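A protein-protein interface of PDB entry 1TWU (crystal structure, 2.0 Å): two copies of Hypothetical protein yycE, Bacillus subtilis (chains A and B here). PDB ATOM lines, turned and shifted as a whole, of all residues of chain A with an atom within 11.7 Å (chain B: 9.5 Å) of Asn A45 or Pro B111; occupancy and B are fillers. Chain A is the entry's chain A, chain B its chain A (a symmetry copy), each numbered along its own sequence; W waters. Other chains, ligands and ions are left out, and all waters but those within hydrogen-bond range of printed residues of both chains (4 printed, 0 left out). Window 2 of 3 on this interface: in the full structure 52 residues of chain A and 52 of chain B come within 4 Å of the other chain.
The side-chain amide oxygen (OD1) of Asn B110 lies within hydrogen-bond range of the side-chain amide nitrogen (ND2) of Asn A45, at 3.3 Å.
The side-chain amide oxygen (OD1) of Asn B110 lies close to the backbone NH (N) of Tyr B112 (3.1 Å). NE2 of His A44 sits at hydrogen-bond distance from ND2 of Asn A45. OE1 of Glu A62 is in salt-bridge range of NH1 of Arg A14, 3.1 Å away. The side-chain hydroxyl (OG) of Ser B108 lies within hydrogen-bond range of the backbone carbonyl oxygen (O) of Asn B110 (3.0 Å).
Arg A14 touches Trp B113. His A44 touches Tyr B112 (NE2 to CD1, 3.8 Å). CG of Pro B111 touches ND2 of Asn A45, 3.7 Å away. Tyr A47 touches Asp B78 (OH to OD2, 3.5 Å). ND2 of Asn B110 touches CD2 of Tyr A47, at 3.2 Å. Glu A62 touches Trp B113.
Of the printed residues of chain B, Asn A45 touches Asn B110 and Pro B111. Pro B111 touches just one residue of chain A: Asn A45. His A44 touches one residue of chain B. Gly A46 touches none of the printed residues of chain B. Asn B110 touches just these residues of chain A: Asn A45 and Tyr A47. No residue of chain A comes within 4 Å of Asn B115. Of the printed residues of chain B, Tyr A47 touches Asp B78 (3.5 Å) and Asn B110 (3.2 Å). Printed residues of chain B within 4 Å of Glu A62: Trp B113 (3.8 Å). The nearest residue of chain A that does not touch Pro B111 is Tyr A47 (5.4 Å).
Of the 16 printed residues of chain B, 5 touch a printed residue of chain A. Printed residues of chain B that touch a printed residue of chain A: Asp B78, Asn B110, Pro B111, Tyr B112 and Trp B113. Hydrophobic or aromatic side chains of chain B within 4 Å of the printed part of chain A: Pro B111, Tyr B112 and Trp B113. Along chain B the printed residues that touch a printed residue of chain A span positions 78 to 113. Along chain A the printed residues that touch a printed residue of chain B span positions 14 to 62. Among the printed residues, no Asp or Glu carboxylate lies within 4 Å of a Lys or Arg side-chain nitrogen of the other chain.
No position is printed for both chains. Of the 7 pairs that touch across the chains among the printed residues, none has its exchanged pair printed and touching as well.
Water W3 lies within hydrogen-bond range of ND2 of Asn B110 (2.6 Å) and O of His A44 (2.8 Å). Water W4 lies within hydrogen-bond range of O of Asp B78 and OG1 of Thr A64. Water W1 bridges NE1 of Trp B113 and OE1 of Glu A62. Water W2 lies within hydrogen-bond range of the side-chain hydroxyl (OG1) of Thr A64 (2.9 Å), the side-chain carboxylate (OD2) of Asp B78 (3.3 Å) and the side-chain hydroxyl (OG) of Ser A70 (3.3 Å).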
ATOM      1  N   ARG A  14     -29.223 -17.564 -14.583  1.00  0.00           N
ATOM      2  CA  ARG A  14     -28.725 -16.774 -15.694  1.00  0.00           C
ATOM      3  C   ARG A  14     -29.819 -15.996 -16.417  1.00  0.00           C
ATOM      4  O   ARG A  14     -30.906 -16.520 -16.673  1.00  0.00           O
ATOM      5  CB  ARG A  14     -28.016 -17.686 -16.705  1.00  0.00           C
ATOM      6  CG  ARG A  14     -27.626 -16.985 -18.008  1.00  0.00           C
ATOM      7  CD  ARG A  14     -27.027 -17.938 -19.026  1.00  0.00           C
ATOM      8  NE  ARG A  14     -25.711 -18.425 -18.614  1.00  0.00           N
ATOM      9  CZ  ARG A  14     -24.969 -19.288 -19.306  1.00  0.00           C
ATOM     10  NH1 ARG A  14     -25.405 -19.772 -20.460  1.00  0.00           N
ATOM     11  NH2 ARG A  14     -23.786 -19.668 -18.843  1.00  0.00           N
ATOM     12  N   GLU A  40     -17.165 -17.184 -21.774  1.00  0.00           N
ATOM     13  CA  GLU A  40     -17.309 -16.710 -23.147  1.00  0.00           C
ATOM     14  C   GLU A  40     -17.195 -17.922 -24.056  1.00  0.00           C
ATOM     15  O   GLU A  40     -16.690 -18.969 -23.653  1.00  0.00           O
ATOM     16  CB  GLU A  40     -16.201 -15.717 -23.508  1.00  0.00           C
ATOM     17  CG  GLU A  40     -14.864 -16.394 -23.787  1.00  0.00           C
ATOM     18  CD  GLU A  40     -13.757 -15.418 -24.133  1.00  0.00           C
ATOM     19  OE1 GLU A  40     -13.359 -14.625 -23.248  1.00  0.00           O
ATOM     20  OE2 GLU A  40     -13.280 -15.444 -25.290  1.00  0.00           O
ATOM     21  N   PHE A  41     -17.674 -17.780 -25.281  1.00  0.00           N
ATOM     22  CA  PHE A  41     -17.600 -18.860 -26.250  1.00  0.00           C
ATOM     23  C   PHE A  41     -17.671 -18.281 -27.655  1.00  0.00           C
ATOM     24  O   PHE A  41     -18.430 -17.341 -27.929  1.00  0.00           O
ATOM     25  CB  PHE A  41     -18.723 -19.882 -26.009  1.00  0.00           C
ATOM     26  CG  PHE A  41     -20.112 -19.341 -26.220  1.00  0.00           C
ATOM     27  CD1 PHE A  41     -20.722 -19.418 -27.469  1.00  0.00           C
ATOM     28  CD2 PHE A  41     -20.828 -18.788 -25.157  1.00  0.00           C
ATOM     29  CE1 PHE A  41     -22.030 -18.959 -27.657  1.00  0.00           C
ATOM     30  CE2 PHE A  41     -22.137 -18.325 -25.333  1.00  0.00           C
ATOM     31  CZ  PHE A  41     -22.738 -18.413 -26.588  1.00  0.00           C
ATOM     32  N   SER A  42     -16.854 -18.835 -28.538  1.00  0.00           N
ATOM     33  CA  SER A  42     -16.802 -18.378 -29.908  1.00  0.00           C
ATOM     34  C   SER A  42     -17.281 -19.488 -30.824  1.00  0.00           C
ATOM     35  O   SER A  42     -16.926 -20.653 -30.637  1.00  0.00           O
ATOM     36  CB  SER A  42     -15.368 -17.990 -30.260  1.00  0.00           C
ATOM     37  OG  SER A  42     -15.302 -17.357 -31.523  1.00  0.00           O
ATOM     38  N   GLN A  43     -18.098 -19.117 -31.802  1.00  0.00           N
ATOM     39  CA  GLN A  43     -18.633 -20.053 -32.785  1.00  0.00           C
ATOM     40  C   GLN A  43     -19.182 -21.370 -32.258  1.00  0.00           C
ATOM     41  O   GLN A  43     -18.622 -22.434 -32.532  1.00  0.00           O
ATOM     42  CB  GLN A  43     -17.573 -20.363 -33.837  1.00  0.00           C
ATOM     43  CG  GLN A  43     -17.212 -19.187 -34.714  1.00  0.00           C
ATOM     44  CD  GLN A  43     -15.985 -19.466 -35.558  1.00  0.00           C
ATOM     45  OE1 GLN A  43     -14.875 -19.600 -35.035  1.00  0.00           O
ATOM     46  NE2 GLN A  43     -16.179 -19.568 -36.873  1.00  0.00           N
ATOM     47  N   HIS A  44     -20.263 -21.308 -31.491  1.00  0.00           N
ATOM     48  CA  HIS A  44     -20.889 -22.531 -31.010  1.00  0.00           C
ATOM     49  C   HIS A  44     -22.303 -22.531 -31.577  1.00  0.00           C
ATOM     50  O   HIS A  44     -23.156 -21.768 -31.134  1.00  0.00           O
ATOM     51  CB  HIS A  44     -20.926 -22.604 -29.477  1.00  0.00           C
ATOM     52  CG  HIS A  44     -21.541 -23.871 -28.961  1.00  0.00           C
ATOM     53  ND1 HIS A  44     -21.083 -25.120 -29.323  1.00  0.00           N
ATOM     54  CD2 HIS A  44     -22.618 -24.084 -28.168  1.00  0.00           C
ATOM     55  CE1 HIS A  44     -21.853 -26.046 -28.781  1.00  0.00           C
ATOM     56  NE2 HIS A  44     -22.794 -25.444 -28.076  1.00  0.00           N
ATOM     57  N   ASN A  45     -22.536 -23.386 -32.568  1.00  0.00           N
ATOM     58  CA  ASN A  45     -23.830 -23.476 -33.233  1.00  0.00           C
ATOM     59  C   ASN A  45     -24.154 -22.144 -33.907  1.00  0.00           C
ATOM     60  O   ASN A  45     -25.319 -21.741 -33.995  1.00  0.00           O
ATOM     61  CB  ASN A  45     -24.943 -23.851 -32.241  1.00  0.00           C
ATOM     62  CG  ASN A  45     -24.762 -25.246 -31.656  1.00  0.00           C
ATOM     63  OD1 ASN A  45     -24.302 -26.165 -32.340  1.00  0.00           O
ATOM     64  ND2 ASN A  45     -25.138 -25.415 -30.389  1.00  0.00           N
ATOM     65  N   GLY A  46     -23.111 -21.466 -34.379  1.00  0.00           N
ATOM     66  CA  GLY A  46     -23.290 -20.193 -35.054  1.00  0.00           C
ATOM     67  C   GLY A  46     -23.419 -19.003 -34.124  1.00  0.00           C
ATOM     68  O   GLY A  46     -23.658 -17.874 -34.569  1.00  0.00           O
ATOM     69  N   TYR A  47     -23.253 -19.249 -32.829  1.00  0.00           N
ATOM     70  CA  TYR A  47     -23.356 -18.194 -31.831  1.00  0.00           C
ATOM     71  C   TYR A  47     -22.038 -17.855 -31.149  1.00  0.00           C
ATOM     72  O   TYR A  47     -21.130 -18.680 -31.036  1.00  0.00           O
ATOM     73  CB  TYR A  47     -24.345 -18.591 -30.739  1.00  0.00           C
ATOM     74  CG  TYR A  47     -25.808 -18.560 -31.114  1.00  0.00           C
ATOM     75  CD1 TYR A  47     -26.541 -17.374 -31.053  1.00  0.00           C
ATOM     76  CD2 TYR A  47     -26.482 -19.735 -31.435  1.00  0.00           C
ATOM     77  CE1 TYR A  47     -27.917 -17.363 -31.286  1.00  0.00           C
ATOM     78  CE2 TYR A  47     -27.852 -19.737 -31.672  1.00  0.00           C
ATOM     79  CZ  TYR A  47     -28.566 -18.551 -31.592  1.00  0.00           C
ATOM     80  OH  TYR A  47     -29.931 -18.572 -31.784  1.00  0.00           O
ATOM     81  N   ASP A  48     -21.967 -16.616 -30.690  1.00  0.00           N
ATOM     82  CA  ASP A  48     -20.831 -16.100 -29.951  1.00  0.00           C
ATOM     83  C   ASP A  48     -21.490 -15.528 -28.705  1.00  0.00           C
ATOM     84  O   ASP A  48     -22.624 -15.059 -28.773  1.00  0.00           O
ATOM     85  CB  ASP A  48     -20.135 -14.992 -30.738  1.00  0.00           C
ATOM     86  CG  ASP A  48     -19.119 -15.530 -31.726  1.00  0.00           C
ATOM     87  OD1 ASP A  48     -19.375 -16.579 -32.358  1.00  0.00           O
ATOM     88  OD2 ASP A  48     -18.059 -14.892 -31.877  1.00  0.00           O
ATOM     89  N   GLY A  49     -20.804 -15.582 -27.570  1.00  0.00           N
ATOM     90  CA  GLY A  49     -21.402 -15.056 -26.358  1.00  0.00           C
ATOM     91  C   GLY A  49     -20.416 -14.776 -25.252  1.00  0.00           C
ATOM     92  O   GLY A  49     -19.262 -15.205 -25.304  1.00  0.00           O
ATOM     93  N   GLU A  62     -25.779 -13.214 -19.526  1.00  0.00           N
ATOM     94  CA  GLU A  62     -25.173 -13.788 -20.720  1.00  0.00           C
ATOM     95  C   GLU A  62     -25.707 -13.020 -21.923  1.00  0.00           C
ATOM     96  O   GLU A  62     -26.894 -12.714 -22.004  1.00  0.00           O
ATOM     97  CB  GLU A  62     -25.503 -15.270 -20.908  1.00  0.00           C
ATOM     98  CG  GLU A  62     -24.971 -15.771 -22.252  1.00  0.00           C
ATOM     99  CD  GLU A  62     -25.420 -17.171 -22.622  1.00  0.00           C
ATOM    100  OE1 GLU A  62     -26.560 -17.549 -22.279  1.00  0.00           O
ATOM    101  OE2 GLU A  62     -24.634 -17.885 -23.282  1.00  0.00           O
ATOM    102  N   THR A  64     -25.652 -13.039 -26.184  1.00  0.00           N
ATOM    103  CA  THR A  64     -25.340 -13.835 -27.359  1.00  0.00           C
ATOM    104  C   THR A  64     -25.661 -13.113 -28.668  1.00  0.00           C
ATOM    105  O   THR A  64     -26.587 -12.304 -28.743  1.00  0.00           O
ATOM    106  CB  THR A  64     -26.104 -15.179 -27.324  1.00  0.00           C
ATOM    107  OG1 THR A  64     -27.515 -14.935 -27.207  1.00  0.00           O
ATOM    108  CG2 THR A  64     -25.640 -16.015 -26.139  1.00  0.00           C
ATOM    109  N   GLN A  65     -24.872 -13.421 -29.694  1.00  0.00           N
ATOM    110  CA  GLN A  65     -25.039 -12.847 -31.021  1.00  0.00           C
ATOM    111  C   GLN A  65     -24.935 -13.966 -32.049  1.00  0.00           C
ATOM    112  O   GLN A  65     -24.003 -14.767 -32.007  1.00  0.00           O
ATOM    113  CB  GLN A  65     -23.953 -11.799 -31.267  1.00  0.00           C
ATOM    114  CG  GLN A  65     -24.003 -11.145 -32.631  1.00  0.00           C
ATOM    115  CD  GLN A  65     -23.020 -10.001 -32.751  1.00  0.00           C
ATOM    116  OE1 GLN A  65     -22.671  -9.579 -33.852  1.00  0.00           O
ATOM    117  NE2 GLN A  65     -22.575  -9.484 -31.620  1.00  0.00           N
ATOM    118  N   TYR A  66     -25.893 -14.025 -32.969  1.00  0.00           N
ATOM    119  CA  TYR A  66     -25.881 -15.061 -33.995  1.00  0.00           C
ATOM    120  C   TYR A  66     -25.095 -14.632 -35.235  1.00  0.00           C
ATOM    121  O   TYR A  66     -25.204 -13.493 -35.684  1.00  0.00           O
ATOM    122  CB  TYR A  66     -27.306 -15.431 -34.385  1.00  0.00           C
ATOM    123  CG  TYR A  66     -27.373 -16.630 -35.298  1.00  0.00           C
ATOM    124  CD1 TYR A  66     -26.851 -17.862 -34.905  1.00  0.00           C
ATOM    125  CD2 TYR A  66     -27.934 -16.527 -36.569  1.00  0.00           C
ATOM    126  CE1 TYR A  66     -26.882 -18.964 -35.758  1.00  0.00           C
ATOM    127  CE2 TYR A  66     -27.970 -17.619 -37.432  1.00  0.00           C
ATOM    128  CZ  TYR A  66     -27.442 -18.834 -37.025  1.00  0.00           C
ATOM    129  OH  TYR A  66     -27.462 -19.905 -37.896  1.00  0.00           O
ATOM    130  N   GLU A  67     -24.300 -15.555 -35.773  1.00  0.00           N
ATOM    131  CA  GLU A  67     -23.477 -15.287 -36.948  1.00  0.00           C
ATOM    132  C   GLU A  67     -24.297 -14.755 -38.114  1.00  0.00           C
ATOM    133  O   GLU A  67     -23.860 -13.853 -38.831  1.00  0.00           O
ATOM    134  CB  GLU A  67     -22.749 -16.555 -37.396  1.00  0.00           C
ATOM    135  CG  GLU A  67     -23.671 -17.736 -37.668  1.00  0.00           C
ATOM    136  CD  GLU A  67     -23.031 -18.807 -38.553  1.00  0.00           C
ATOM    137  OE1 GLU A  67     -21.791 -18.974 -38.498  1.00  0.00           O
ATOM    138  OE2 GLU A  67     -23.774 -19.492 -39.296  1.00  0.00           O
ATOM    139  N   GLY A  68     -25.481 -15.325 -38.306  1.00  0.00           N
ATOM    140  CA  GLY A  68     -26.339 -14.886 -39.390  1.00  0.00           C
ATOM    141  C   GLY A  68     -27.231 -13.725 -38.985  1.00  0.00           C
ATOM    142  O   GLY A  68     -28.429 -13.722 -39.268  1.00  0.00           O
ATOM    143  N   GLY A  69     -26.648 -12.738 -38.315  1.00  0.00           N
ATOM    144  CA  GLY A  69     -27.421 -11.587 -37.891  1.00  0.00           C
ATOM    145  C   GLY A  69     -28.317 -11.888 -36.706  1.00  0.00           C
ATOM    146  O   GLY A  69     -29.014 -12.904 -36.675  1.00  0.00           O
ATOM    147  N   SER A  70     -28.295 -10.994 -35.727  1.00  0.00           N
ATOM    148  CA  SER A  70     -29.099 -11.158 -34.530  1.00  0.00           C
ATOM    149  C   SER A  70     -29.573  -9.783 -34.075  1.00  0.00           C
ATOM    150  O   SER A  70     -28.906  -8.779 -34.316  1.00  0.00           O
ATOM    151  CB  SER A  70     -28.256 -11.816 -33.433  1.00  0.00           C
ATOM    152  OG  SER A  70     -29.058 -12.213 -32.334  1.00  0.00           O
ATOM    153  N   PRO B  77     -37.096 -15.142 -28.766  1.00  0.00           N
ATOM    154  CA  PRO B  77     -36.777 -16.538 -28.461  1.00  0.00           C
ATOM    155  C   PRO B  77     -35.417 -16.759 -27.813  1.00  0.00           C
ATOM    156  O   PRO B  77     -35.155 -17.833 -27.278  1.00  0.00           O
ATOM    157  CB  PRO B  77     -36.898 -17.217 -29.820  1.00  0.00           C
ATOM    158  CG  PRO B  77     -36.489 -16.140 -30.768  1.00  0.00           C
ATOM    159  CD  PRO B  77     -37.213 -14.938 -30.222  1.00  0.00           C
ATOM    160  N   ASP B  78     -34.557 -15.745 -27.866  1.00  0.00           N
ATOM    161  CA  ASP B  78     -33.228 -15.829 -27.271  1.00  0.00           C
ATOM    162  C   ASP B  78     -33.126 -15.075 -25.942  1.00  0.00           C
ATOM    163  O   ASP B  78     -32.046 -14.973 -25.357  1.00  0.00           O
ATOM    164  CB  ASP B  78     -32.168 -15.286 -28.234  1.00  0.00           C
ATOM    165  CG  ASP B  78     -31.929 -16.199 -29.421  1.00  0.00           C
ATOM    166  OD1 ASP B  78     -32.187 -17.414 -29.303  1.00  0.00           O
ATOM    167  OD2 ASP B  78     -31.458 -15.702 -30.467  1.00  0.00           O
ATOM    168  N   GLU B 107     -39.467 -25.346 -28.210  1.00  0.00           N
ATOM    169  CA  GLU B 107     -38.182 -25.776 -28.726  1.00  0.00           C
ATOM    170  C   GLU B 107     -37.238 -24.582 -28.678  1.00  0.00           C
ATOM    171  O   GLU B 107     -37.460 -23.576 -29.352  1.00  0.00           O
ATOM    172  CB  GLU B 107     -38.341 -26.253 -30.166  1.00  0.00           C
ATOM    173  CG  GLU B 107     -37.396 -27.369 -30.532  1.00  0.00           C
ATOM    174  CD  GLU B 107     -37.640 -28.601 -29.688  1.00  0.00           C
ATOM    175  OE1 GLU B 107     -38.614 -29.344 -29.968  1.00  0.00           O
ATOM    176  OE2 GLU B 107     -36.862 -28.812 -28.729  1.00  0.00           O
ATOM    177  N   SER B 108     -36.189 -24.688 -27.872  1.00  0.00           N
ATOM    178  CA  SER B 108     -35.230 -23.602 -27.743  1.00  0.00           C
ATOM    179  C   SER B 108     -34.633 -23.241 -29.093  1.00  0.00           C
ATOM    180  O   SER B 108     -34.521 -24.092 -29.983  1.00  0.00           O
ATOM    181  CB  SER B 108     -34.115 -23.999 -26.774  1.00  0.00           C
ATOM    182  OG  SER B 108     -33.529 -25.231 -27.156  1.00  0.00           O
ATOM    183  N   GLU B 109     -34.269 -21.971 -29.247  1.00  0.00           N
ATOM    184  CA  GLU B 109     -33.666 -21.501 -30.486  1.00  0.00           C
ATOM    185  C   GLU B 109     -32.334 -22.203 -30.661  1.00  0.00           C
ATOM    186  O   GLU B 109     -32.068 -22.832 -31.693  1.00  0.00           O
ATOM    187  CB  GLU B 109     -33.448 -19.992 -30.431  1.00  0.00           C
ATOM    188  CG  GLU B 109     -34.672 -19.200 -30.805  1.00  0.00           C
ATOM    189  CD  GLU B 109     -35.053 -19.383 -32.262  1.00  0.00           C
ATOM    190  OE1 GLU B 109     -34.318 -18.875 -33.139  1.00  0.00           O
ATOM    191  OE2 GLU B 109     -36.083 -20.040 -32.526  1.00  0.00           O
ATOM    192  N   ASN B 110     -31.501 -22.088 -29.632  1.00  0.00           N
ATOM    193  CA  ASN B 110     -30.186 -22.709 -29.620  1.00  0.00           C
ATOM    194  C   ASN B 110     -30.370 -24.178 -29.241  1.00  0.00           C
ATOM    195  O   ASN B 110     -30.820 -24.489 -28.134  1.00  0.00           O
ATOM    196  CB  ASN B 110     -29.299 -22.019 -28.584  1.00  0.00           C
ATOM    197  CG  ASN B 110     -27.831 -22.263 -28.826  1.00  0.00           C
ATOM    198  OD1 ASN B 110     -27.412 -23.382 -29.131  1.00  0.00           O
ATOM    199  ND2 ASN B 110     -27.031 -21.210 -28.684  1.00  0.00           N
ATOM    200  N   PRO B 111     -30.030 -25.101 -30.154  1.00  0.00           N
ATOM    201  CA  PRO B 111     -30.176 -26.534 -29.873  1.00  0.00           C
ATOM    202  C   PRO B 111     -29.420 -26.938 -28.607  1.00  0.00           C
ATOM    203  O   PRO B 111     -29.618 -28.027 -28.063  1.00  0.00           O
ATOM    204  CB  PRO B 111     -29.615 -27.188 -31.134  1.00  0.00           C
ATOM    205  CG  PRO B 111     -28.576 -26.204 -31.577  1.00  0.00           C
ATOM    206  CD  PRO B 111     -29.287 -24.886 -31.407  1.00  0.00           C
ATOM    207  N   TYR B 112     -28.557 -26.036 -28.149  1.00  0.00           N
ATOM    208  CA  TYR B 112     -27.757 -26.245 -26.951  1.00  0.00           C
ATOM    209  C   TYR B 112     -28.640 -26.455 -25.723  1.00  0.00           C
ATOM    210  O   TYR B 112     -28.487 -27.446 -25.005  1.00  0.00           O
ATOM    211  CB  TYR B 112     -26.840 -25.040 -26.716  1.00  0.00           C
ATOM    212  CG  TYR B 112     -26.155 -25.061 -25.372  1.00  0.00           C
ATOM    213  CD1 TYR B 112     -25.091 -25.926 -25.120  1.00  0.00           C
ATOM    214  CD2 TYR B 112     -26.609 -24.254 -24.332  1.00  0.00           C
ATOM    215  CE1 TYR B 112     -24.495 -25.988 -23.860  1.00  0.00           C
ATOM    216  CE2 TYR B 112     -26.026 -24.308 -23.069  1.00  0.00           C
ATOM    217  CZ  TYR B 112     -24.972 -25.177 -22.838  1.00  0.00           C
ATOM    218  OH  TYR B 112     -24.410 -25.233 -21.583  1.00  0.00           O
ATOM    219  N   TRP B 113     -29.558 -25.522 -25.477  1.00  0.00           N
ATOM    220  CA  TRP B 113     -30.445 -25.627 -24.324  1.00  0.00           C
ATOM    221  C   TRP B 113     -31.382 -26.817 -24.467  1.00  0.00           C
ATOM    222  O   TRP B 113     -32.095 -27.185 -23.531  1.00  0.00           O
ATOM    223  CB  TRP B 113     -31.254 -24.342 -24.158  1.00  0.00           C
ATOM    224  CG  TRP B 113     -30.401 -23.146 -23.928  1.00  0.00           C
ATOM    225  CD1 TRP B 113     -30.091 -22.177 -24.834  1.00  0.00           C
ATOM    226  CD2 TRP B 113     -29.710 -22.805 -22.721  1.00  0.00           C
ATOM    227  NE1 TRP B 113     -29.248 -21.250 -24.267  1.00  0.00           N
ATOM    228  CE2 TRP B 113     -28.997 -21.613 -22.970  1.00  0.00           C
ATOM    229  CE3 TRP B 113     -29.623 -23.393 -21.453  1.00  0.00           C
ATOM    230  CZ2 TRP B 113     -28.204 -20.995 -21.997  1.00  0.00           C
ATOM    231  CZ3 TRP B 113     -28.834 -22.779 -20.484  1.00  0.00           C
ATOM    232  CH2 TRP B 113     -28.135 -21.590 -20.765  1.00  0.00           C
ATOM    233  N   SER B 114     -31.372 -27.416 -25.652  1.00  0.00           N
ATOM    234  CA  SER B 114     -32.202 -28.571 -25.934  1.00  0.00           C
ATOM    235  C   SER B 114     -31.531 -29.831 -25.390  1.00  0.00           C
ATOM    236  O   SER B 114     -32.185 -30.849 -25.165  1.00  0.00           O
ATOM    237  CB  SER B 114     -32.416 -28.696 -27.437  1.00  0.00           C
ATOM    238  OG  SER B 114     -33.260 -29.792 -27.722  1.00  0.00           O
ATOM    239  N   ASN B 115     -30.217 -29.752 -25.185  1.00  0.00           N
ATOM    240  CA  ASN B 115     -29.457 -30.876 -24.646  1.00  0.00           C
ATOM    241  C   ASN B 115     -29.521 -30.848 -23.126  1.00  0.00           C
ATOM    242  O   ASN B 115     -28.716 -30.179 -22.479  1.00  0.00           O
ATOM    243  CB  ASN B 115     -27.982 -30.818 -25.074  1.00  0.00           C
ATOM    244  CG  ASN B 115     -27.765 -31.230 -26.526  1.00  0.00           C
ATOM    245  OD1 ASN B 115     -28.476 -32.091 -27.058  1.00  0.00           O
ATOM    246  ND2 ASN B 115     -26.761 -30.631 -27.167  1.00  0.00           N
ATOM    247  N   GLY B 116     -30.480 -31.570 -22.560  1.00  0.00           N
ATOM    248  CA  GLY B 116     -30.602 -31.608 -21.115  1.00  0.00           C
ATOM    249  C   GLY B 116     -31.261 -30.384 -20.510  1.00  0.00           C
ATOM    250  O   GLY B 116     -31.020 -30.054 -19.345  1.00  0.00           O
ATOM    251  N   GLY B 117     -32.093 -29.711 -21.301  1.00  0.00           N
ATOM    252  CA  GLY B 117     -32.783 -28.536 -20.814  1.00  0.00           C
ATOM    253  C   GLY B 117     -34.217 -28.496 -21.302  1.00  0.00           C
ATOM    254  O   GLY B 117     -34.522 -29.027 -22.373  1.00  0.00           O
ATOM    255  N   VAL B 118     -35.100 -27.885 -20.512  1.00  0.00           N
ATOM    256  CA  VAL B 118     -36.512 -27.757 -20.866  1.00  0.00           C
ATOM    257  C   VAL B 118     -36.904 -26.285 -20.824  1.00  0.00           C
ATOM    258  O   VAL B 118     -36.677 -25.608 -19.822  1.00  0.00           O
ATOM    259  CB  VAL B 118     -37.422 -28.527 -19.883  1.00  0.00           C
ATOM    260  CG1 VAL B 118     -38.888 -28.278 -20.224  1.00  0.00           C
ATOM    261  CG2 VAL B 118     -37.111 -30.015 -19.939  1.00  0.00           C
ATOM    262  N   THR B 119     -37.496 -25.794 -21.909  1.00  0.00           N
ATOM    263  CA  THR B 119     -37.918 -24.400 -21.991  1.00  0.00           C
ATOM    264  C   THR B 119     -39.437 -24.274 -21.957  1.00  0.00           C
ATOM    265  O   THR B 119     -40.141 -24.870 -22.771  1.00  0.00           O
ATOM    266  CB  THR B 119     -37.401 -23.731 -23.281  1.00  0.00           C
ATOM    267  OG1 THR B 119     -35.974 -23.836 -23.333  1.00  0.00           O
ATOM    268  CG2 THR B 119     -37.798 -22.257 -23.313  1.00  0.00           C
ATOM    269  N   MET B 131     -32.170 -26.045 -16.901  1.00  0.00           N
ATOM    270  CA  MET B 131     -31.032 -26.810 -17.399  1.00  0.00           C
ATOM    271  C   MET B 131     -30.496 -27.777 -16.344  1.00  0.00           C
ATOM    272  O   MET B 131     -30.232 -27.398 -15.196  1.00  0.00           O
ATOM    273  CB  MET B 131     -29.929 -25.847 -17.864  1.00  0.00           C
ATOM    274  CG  MET B 131     -28.696 -26.507 -18.495  1.00  0.00           C
ATOM    275  SD  MET B 131     -29.013 -27.584 -19.919  1.00  0.00           S
ATOM    276  CE  MET B 131     -29.781 -26.469 -21.035  1.00  0.00           C
HETATM  277  O   HOH W   1     -28.577 -18.502 -24.480  1.00  0.00           O
HETATM  278  O   HOH W   2     -28.546 -14.317 -29.819  1.00  0.00           O
HETATM  279  O   HOH W   3     -24.520 -21.916 -28.662  1.00  0.00           O
HETATM  280  O   HOH W   4     -29.562 -15.868 -25.384  1.00  0.00           O
